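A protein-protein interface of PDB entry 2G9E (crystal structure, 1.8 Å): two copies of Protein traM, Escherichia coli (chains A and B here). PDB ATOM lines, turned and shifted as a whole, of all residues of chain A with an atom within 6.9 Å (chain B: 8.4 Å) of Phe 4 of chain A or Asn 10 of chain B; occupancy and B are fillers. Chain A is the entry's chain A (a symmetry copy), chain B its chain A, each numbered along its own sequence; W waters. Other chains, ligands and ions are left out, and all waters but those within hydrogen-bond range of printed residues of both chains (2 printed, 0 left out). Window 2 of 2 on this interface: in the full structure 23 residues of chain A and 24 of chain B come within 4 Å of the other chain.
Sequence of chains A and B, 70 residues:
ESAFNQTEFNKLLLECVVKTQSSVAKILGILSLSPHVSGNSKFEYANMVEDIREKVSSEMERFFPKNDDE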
ATOM      1  N   ALA A   3      17.774  -1.562   5.449  1.00  0.00           N
ATOM      2  CA  ALA A   3      17.178  -0.200   5.442  1.00  0.00           C
ATOM      3  C   ALA A   3      17.531   0.534   6.740  1.00  0.00           C
ATOM      4  O   ALA A   3      17.278   0.036   7.841  1.00  0.00           O
ATOM      5  CB  ALA A   3      15.672  -0.270   5.231  1.00  0.00           C
ATOM      6  N   PHE A   4      18.165   1.697   6.611  1.00  0.00           N
ATOM      7  CA  PHE A   4      18.621   2.435   7.790  1.00  0.00           C
ATOM      8  C   PHE A   4      17.761   3.676   7.883  1.00  0.00           C
ATOM      9  O   PHE A   4      17.651   4.448   6.928  1.00  0.00           O
ATOM     10  CB  PHE A   4      20.135   2.732   7.716  1.00  0.00           C
ATOM     11  CG  PHE A   4      20.642   3.695   8.773  1.00  0.00           C
ATOM     12  CD1 PHE A   4      21.104   3.225  10.003  1.00  0.00           C
ATOM     13  CD2 PHE A   4      20.686   5.077   8.516  1.00  0.00           C
ATOM     14  CE1 PHE A   4      21.565   4.122  10.984  1.00  0.00           C
ATOM     15  CE2 PHE A   4      21.148   5.979   9.482  1.00  0.00           C
ATOM     16  CZ  PHE A   4      21.586   5.503  10.715  1.00  0.00           C
ATOM     17  N   ASN A   5      17.124   3.836   9.031  1.00  0.00           N
ATOM     18  CA  ASN A   5      16.207   4.925   9.245  1.00  0.00           C
ATOM     19  C   ASN A   5      16.919   5.967  10.095  1.00  0.00           C
ATOM     20  O   ASN A   5      17.025   5.818  11.315  1.00  0.00           O
ATOM     21  CB  ASN A   5      14.943   4.406   9.943  1.00  0.00           C
ATOM     22  CG  ASN A   5      13.843   5.440  10.018  1.00  0.00           C
ATOM     23  OD1 ASN A   5      14.098   6.641  10.080  1.00  0.00           O
ATOM     24  ND2 ASN A   5      12.598   4.971  10.046  1.00  0.00           N
ATOM     25  N   GLN A   6      17.429   6.999   9.428  1.00  0.00           N
ATOM     26  CA  GLN A   6      18.160   8.082  10.095  1.00  0.00           C
ATOM     27  C   GLN A   6      17.300   8.783  11.147  1.00  0.00           C
ATOM     28  O   GLN A   6      17.809   9.171  12.201  1.00  0.00           O
ATOM     29  CB  GLN A   6      18.656   9.116   9.077  1.00  0.00           C
ATOM     30  CG  GLN A   6      19.483  10.239   9.686  1.00  0.00           C
ATOM     31  CD  GLN A   6      20.888   9.776  10.023  1.00  0.00           C
ATOM     32  OE1 GLN A   6      21.619   9.303   9.151  1.00  0.00           O
ATOM     33  NE2 GLN A   6      21.271   9.905  11.290  1.00  0.00           N
ATOM     34  N   THR A   7      16.011   8.982  10.851  1.00  0.00           N
ATOM     35  CA  THR A   7      15.122   9.665  11.813  1.00  0.00           C
ATOM     36  C   THR A   7      14.947   8.835  13.103  1.00  0.00           C
ATOM     37  O   THR A   7      15.044   9.354  14.226  1.00  0.00           O
ATOM     38  CB  THR A   7      13.760  10.068  11.169  1.00  0.00           C
ATOM     39  OG1 THR A   7      14.001  11.007  10.108  1.00  0.00           O
ATOM     40  CG2 THR A   7      12.823  10.714  12.200  1.00  0.00           C
ATOM     41  N   PHE A   9      17.041   6.443  14.102  1.00  0.00           N
ATOM     42  CA  PHE A   9      18.392   6.525  14.691  1.00  0.00           C
ATOM     43  C   PHE A   9      18.568   7.788  15.528  1.00  0.00           C
ATOM     44  O   PHE A   9      18.976   7.713  16.683  1.00  0.00           O
ATOM     45  CB  PHE A   9      19.471   6.496  13.589  1.00  0.00           C
ATOM     46  CG  PHE A   9      20.887   6.432  14.119  1.00  0.00           C
ATOM     47  CD1 PHE A   9      21.478   5.203  14.407  1.00  0.00           C
ATOM     48  CD2 PHE A   9      21.625   7.606  14.324  1.00  0.00           C
ATOM     49  CE1 PHE A   9      22.786   5.128  14.893  1.00  0.00           C
ATOM     50  CE2 PHE A   9      22.930   7.548  14.813  1.00  0.00           C
ATOM     51  CZ  PHE A   9      23.517   6.310  15.099  1.00  0.00           C
ATOM     52  N   ASN A  10      18.253   8.939  14.948  1.00  0.00           N
ATOM     53  CA  ASN A  10      18.295  10.219  15.668  1.00  0.00           C
ATOM     54  C   ASN A  10      17.467  10.216  16.960  1.00  0.00           C
ATOM     55  O   ASN A  10      17.914  10.735  17.984  1.00  0.00           O
ATOM     56  CB  ASN A  10      17.849  11.372  14.758  1.00  0.00           C
ATOM     57  CG  ASN A  10      18.879  11.713  13.683  1.00  0.00           C
ATOM     58  OD1 ASN A  10      20.045  11.290  13.762  1.00  0.00           O
ATOM     59  ND2 ASN A  10      18.464  12.510  12.696  1.00  0.00           N
ATOM     60  N   PHE B   4      36.797   7.869   6.151  1.00  0.00           N
ATOM     61  CA  PHE B   4      35.899   7.934   7.305  1.00  0.00           C
ATOM     62  C   PHE B   4      34.648   7.174   6.923  1.00  0.00           C
ATOM     63  O   PHE B   4      34.023   7.449   5.897  1.00  0.00           O
ATOM     64  CB  PHE B   4      35.633   9.396   7.729  1.00  0.00           C
ATOM     65  CG  PHE B   4      34.532   9.563   8.758  1.00  0.00           C
ATOM     66  CD1 PHE B   4      34.821   9.541  10.123  1.00  0.00           C
ATOM     67  CD2 PHE B   4      33.202   9.780   8.351  1.00  0.00           C
ATOM     68  CE1 PHE B   4      33.794   9.689  11.074  1.00  0.00           C
ATOM     69  CE2 PHE B   4      32.173   9.934   9.288  1.00  0.00           C
ATOM     70  CZ  PHE B   4      32.469   9.888  10.648  1.00  0.00           C
ATOM     71  N   ASN B   5      34.313   6.190   7.742  1.00  0.00           N
ATOM     72  CA  ASN B   5      33.195   5.325   7.473  1.00  0.00           C
ATOM     73  C   ASN B   5      32.048   5.762   8.371  1.00  0.00           C
ATOM     74  O   ASN B   5      32.017   5.430   9.559  1.00  0.00           O
ATOM     75  CB  ASN B   5      33.591   3.867   7.745  1.00  0.00           C
ATOM     76  CG  ASN B   5      32.546   2.877   7.289  1.00  0.00           C
ATOM     77  OD1 ASN B   5      31.352   3.168   7.276  1.00  0.00           O
ATOM     78  ND2 ASN B   5      32.991   1.672   6.940  1.00  0.00           N
ATOM     79  N   GLN B   6      31.130   6.535   7.795  1.00  0.00           N
ATOM     80  CA  GLN B   6      29.970   7.055   8.525  1.00  0.00           C
ATOM     81  C   GLN B   6      29.112   5.929   9.104  1.00  0.00           C
ATOM     82  O   GLN B   6      28.579   6.065  10.208  1.00  0.00           O
ATOM     83  CB  GLN B   6      29.102   7.936   7.618  1.00  0.00           C
ATOM     84  CG  GLN B   6      27.911   8.568   8.323  1.00  0.00           C
ATOM     85  CD  GLN B   6      28.336   9.738   9.191  1.00  0.00           C
ATOM     86  OE1 GLN B   6      28.940  10.695   8.703  1.00  0.00           O
ATOM     87  NE2 GLN B   6      28.026   9.666  10.482  1.00  0.00           N
ATOM     88  N   THR B   7      28.945   4.837   8.350  1.00  0.00           N
ATOM     89  CA  THR B   7      28.118   3.714   8.838  1.00  0.00           C
ATOM     90  C   THR B   7      28.747   3.053  10.083  1.00  0.00           C
ATOM     91  O   THR B   7      28.070   2.787  11.087  1.00  0.00           O
ATOM     92  CB  THR B   7      27.798   2.687   7.708  1.00  0.00           C
ATOM     93  OG1 THR B   7      27.027   3.338   6.685  1.00  0.00           O
ATOM     94  CG2 THR B   7      26.997   1.494   8.248  1.00  0.00           C
ATOM     95  N   GLU B   8      30.051   2.806  10.016  1.00  0.00           N
ATOM     96  CA  GLU B   8      30.793   2.263  11.168  1.00  0.00           C
ATOM     97  C   GLU B   8      30.842   3.225  12.351  1.00  0.00           C
ATOM     98  O   GLU B   8      30.760   2.787  13.490  1.00  0.00           O
ATOM     99  CB  GLU B   8      32.199   1.857  10.777  1.00  0.00           C
ATOM    100  CG  GLU B   8      32.234   0.648   9.838  1.00  0.00           C
ATOM    101  CD  GLU B   8      31.604  -0.585  10.452  1.00  0.00           C
ATOM    102  OE1 GLU B   8      31.948  -0.924  11.605  1.00  0.00           O
ATOM    103  OE2 GLU B   8      30.759  -1.209   9.778  1.00  0.00           O
ATOM    104  N   PHE B   9      30.989   4.519  12.064  1.00  0.00           N
ATOM    105  CA  PHE B   9      30.837   5.585  13.073  1.00  0.00           C
ATOM    106  C   PHE B   9      29.467   5.538  13.742  1.00  0.00           C
ATOM    107  O   PHE B   9      29.377   5.516  14.966  1.00  0.00           O
ATOM    108  CB  PHE B   9      31.041   6.974  12.435  1.00  0.00           C
ATOM    109  CG  PHE B   9      31.042   8.112  13.433  1.00  0.00           C
ATOM    110  CD1 PHE B   9      32.222   8.490  14.071  1.00  0.00           C
ATOM    111  CD2 PHE B   9      29.859   8.805  13.725  1.00  0.00           C
ATOM    112  CE1 PHE B   9      32.239   9.542  14.991  1.00  0.00           C
ATOM    113  CE2 PHE B   9      29.859   9.854  14.645  1.00  0.00           C
ATOM    114  CZ  PHE B   9      31.048  10.228  15.281  1.00  0.00           C
ATOM    115  N   ASN B  10      28.411   5.516  12.940  1.00  0.00           N
ATOM    116  CA  ASN B  10      27.039   5.385  13.452  1.00  0.00           C
ATOM    117  C   ASN B  10      26.843   4.162  14.358  1.00  0.00           C
ATOM    118  O   ASN B  10      26.185   4.259  15.394  1.00  0.00           O
ATOM    119  CB  ASN B  10      26.028   5.354  12.297  1.00  0.00           C
ATOM    120  CG  ASN B  10      25.860   6.712  11.618  1.00  0.00           C
ATOM    121  OD1 ASN B  10      26.279   7.750  12.157  1.00  0.00           O
ATOM    122  ND2 ASN B  10      25.211   6.714  10.451  1.00  0.00           N
ATOM    123  N   LYS B  11      27.418   3.024  13.958  1.00  0.00           N
ATOM    124  CA  LYS B  11      27.320   1.753  14.708  1.00  0.00           C
ATOM    125  C   LYS B  11      28.020   1.872  16.049  1.00  0.00           C
ATOM    126  O   LYS B  11      27.462   1.483  17.068  1.00  0.00           O
ATOM    127  CB  LYS B  11      27.965   0.601  13.948  1.00  0.00           C
ATOM    128  CG  LYS B  11      27.161   0.102  12.786  1.00  0.00           C
ATOM    129  CD  LYS B  11      27.878  -0.948  11.941  1.00  0.00           C
ATOM    130  CE  LYS B  11      28.252  -2.196  12.734  1.00  0.00           C
ATOM    131  NZ  LYS B  11      28.870  -3.194  11.784  1.00  0.00           N
ATOM    132  N   LEU B  12      29.242   2.415  16.042  1.00  0.00           N
ATOM    133  CA  LEU B  12      29.966   2.649  17.306  1.00  0.00           C
ATOM    134  C   LEU B  12      29.254   3.648  18.213  1.00  0.00           C
ATOM    135  O   LEU B  12      29.169   3.419  19.421  1.00  0.00           O
ATOM    136  CB  LEU B  12      31.417   3.095  17.085  1.00  0.00           C
ATOM    137  CG  LEU B  12      32.224   3.375  18.379  1.00  0.00           C
ATOM    138  CD1 LEU B  12      32.384   2.111  19.181  1.00  0.00           C
ATOM    139  CD2 LEU B  12      33.569   3.945  18.048  1.00  0.00           C
ATOM    140  N   LEU B  13      28.784   4.757  17.639  1.00  0.00           N
ATOM    141  CA  LEU B  13      28.027   5.766  18.376  1.00  0.00           C
ATOM    142  C   LEU B  13      26.832   5.117  19.061  1.00  0.00           C
ATOM    143  O   LEU B  13      26.601   5.314  20.253  1.00  0.00           O
ATOM    144  CB  LEU B  13      27.556   6.886  17.441  1.00  0.00           C
ATOM    145  CG  LEU B  13      26.732   8.044  18.030  1.00  0.00           C
ATOM    146  CD1 LEU B  13      27.444   8.715  19.230  1.00  0.00           C
ATOM    147  CD2 LEU B  13      26.421   9.106  16.952  1.00  0.00           C
ATOM    148  N   LEU B  14      26.075   4.330  18.307  1.00  0.00           N
ATOM    149  CA  LEU B  14      24.877   3.709  18.838  1.00  0.00           C
ATOM    150  C   LEU B  14      25.192   2.704  19.937  1.00  0.00           C
ATOM    151  O   LEU B  14      24.530   2.682  20.968  1.00  0.00           O
ATOM    152  CB  LEU B  14      24.066   3.055  17.707  1.00  0.00           C
ATOM    153  CG  LEU B  14      22.590   2.901  18.070  1.00  0.00           C
ATOM    154  CD1 LEU B  14      21.866   4.294  18.202  1.00  0.00           C
ATOM    155  CD2 LEU B  14      21.876   1.958  17.118  1.00  0.00           C
ATOM    156  N   GLU B  15      26.177   1.846  19.704  1.00  0.00           N
ATOM    157  CA  GLU B  15      26.559   0.863  20.705  1.00  0.00           C
ATOM    158  C   GLU B  15      26.943   1.537  22.033  1.00  0.00           C
ATOM    159  O   GLU B  15      26.483   1.122  23.082  1.00  0.00           O
ATOM    160  CB  GLU B  15      27.724   0.049  20.203  1.00  0.00           C
ATOM    161  CG  GLU B  15      28.239  -0.941  21.216  1.00  0.00           C
ATOM    162  CD  GLU B  15      29.439  -1.671  20.709  1.00  0.00           C
ATOM    163  OE1 GLU B  15      30.457  -1.024  20.406  1.00  0.00           O
ATOM    164  OE2 GLU B  15      29.363  -2.899  20.606  1.00  0.00           O
ATOM    165  N   CYS B  16      27.781   2.565  21.960  1.00  0.00           N
ATOM    166  CA  CYS B  16      28.254   3.265  23.152  1.00  0.00           C
ATOM    167  C   CYS B  16      27.076   3.866  23.916  1.00  0.00           C
ATOM    168  O   CYS B  16      26.949   3.649  25.145  1.00  0.00           O
ATOM    169  CB  CYS B  16      29.233   4.380  22.794  1.00  0.00           C
ATOM    170  SG  CYS B  16      30.850   3.807  22.295  1.00  0.00           S
ATOM    171  N   VAL B  17      26.229   4.621  23.212  1.00  0.00           N
ATOM    172  CA  VAL B  17      25.147   5.309  23.920  1.00  0.00           C
ATOM    173  C   VAL B  17      24.095   4.335  24.465  1.00  0.00           C
ATOM    174  O   VAL B  17      23.562   4.572  25.537  1.00  0.00           O
ATOM    175  CB  VAL B  17      24.523   6.513  23.133  1.00  0.00           C
ATOM    176  CG1 VAL B  17      25.612   7.502  22.704  1.00  0.00           C
ATOM    177  CG2 VAL B  17      23.651   6.068  21.947  1.00  0.00           C
HETATM  178  O   HOH W   1      24.173  10.101  12.369  1.00  0.00           O
HETATM  179  O   HOH W   2      24.407   9.256   9.231  1.00  0.00           O
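The side-chain amide oxygen (OD1) of Asn 10 of chain B is in hydrogen-bond range of the side-chain amide nitrogen (NE2) of Gln 6 of chain B.
Among the printed residues, merely in contact across the chains: Phe 9 of chain A with Asn 10 of chain B (3.4 Å), Phe 9 of chain A with Leu 14 of chain B (3.5 Å) and Phe 4 of chain A with Asn 10 of chain B (3.8 Å).
Asn 10 of chain B touches just these residues of chain A: Phe 4 and Phe 9. No residue of chain B comes within 4 Å of Ala 3 of chain A. Printed residues of chain A within 4 Å of Leu 14 of chain B: Phe 9. Printed residues of chain B within 4 Å of Phe 9 of chain A: Asn 10 (3.4 Å) and Leu 14 (3.5 Å).
Water W2 lies within hydrogen-bond range of OE1 of Gln 6 of chain A (2.8 Å) and ND2 of Asn 10 of chain B (2.9 Å). Water W1 lies within hydrogen-bond range of the side-chain amide nitrogen (NE2) of Gln 6 of chain A and the side-chain amide oxygen (OD1) of Asn 10 of chain B.
Of the 14 printed residues of chain B, 2 touch a printed residue of chain A. Of the 7 printed residues of chain A, 2 touch a printed residue of chain B. Printed residues of chain A that touch a printed residue of chain B: Phe 4 and Phe 9. Hydrophobic or aromatic side chains of chain A within 4 Å of the printed part of chain B: Phe 4 and Phe 9. Among the printed residues, no Asp or Glu carboxylate lies within 4 Å of a Lys or Arg side-chain nitrogen of the other chain.
Phe 4 of chain A touches Asn 10 of chain B, but with the chains exchanged Asn 10 of chain A does not touch Phe 4 of chain B (12.9 Å). Phe 9 of chain A touches Asn 10 of chain B, but with the chains exchanged Asn 10 of chain A does not touch Phe 9 of chain B (10.0 Å). Of the 3 pairs that touch across the chains among the printed residues, none has its exchanged pair printed and touching as well.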
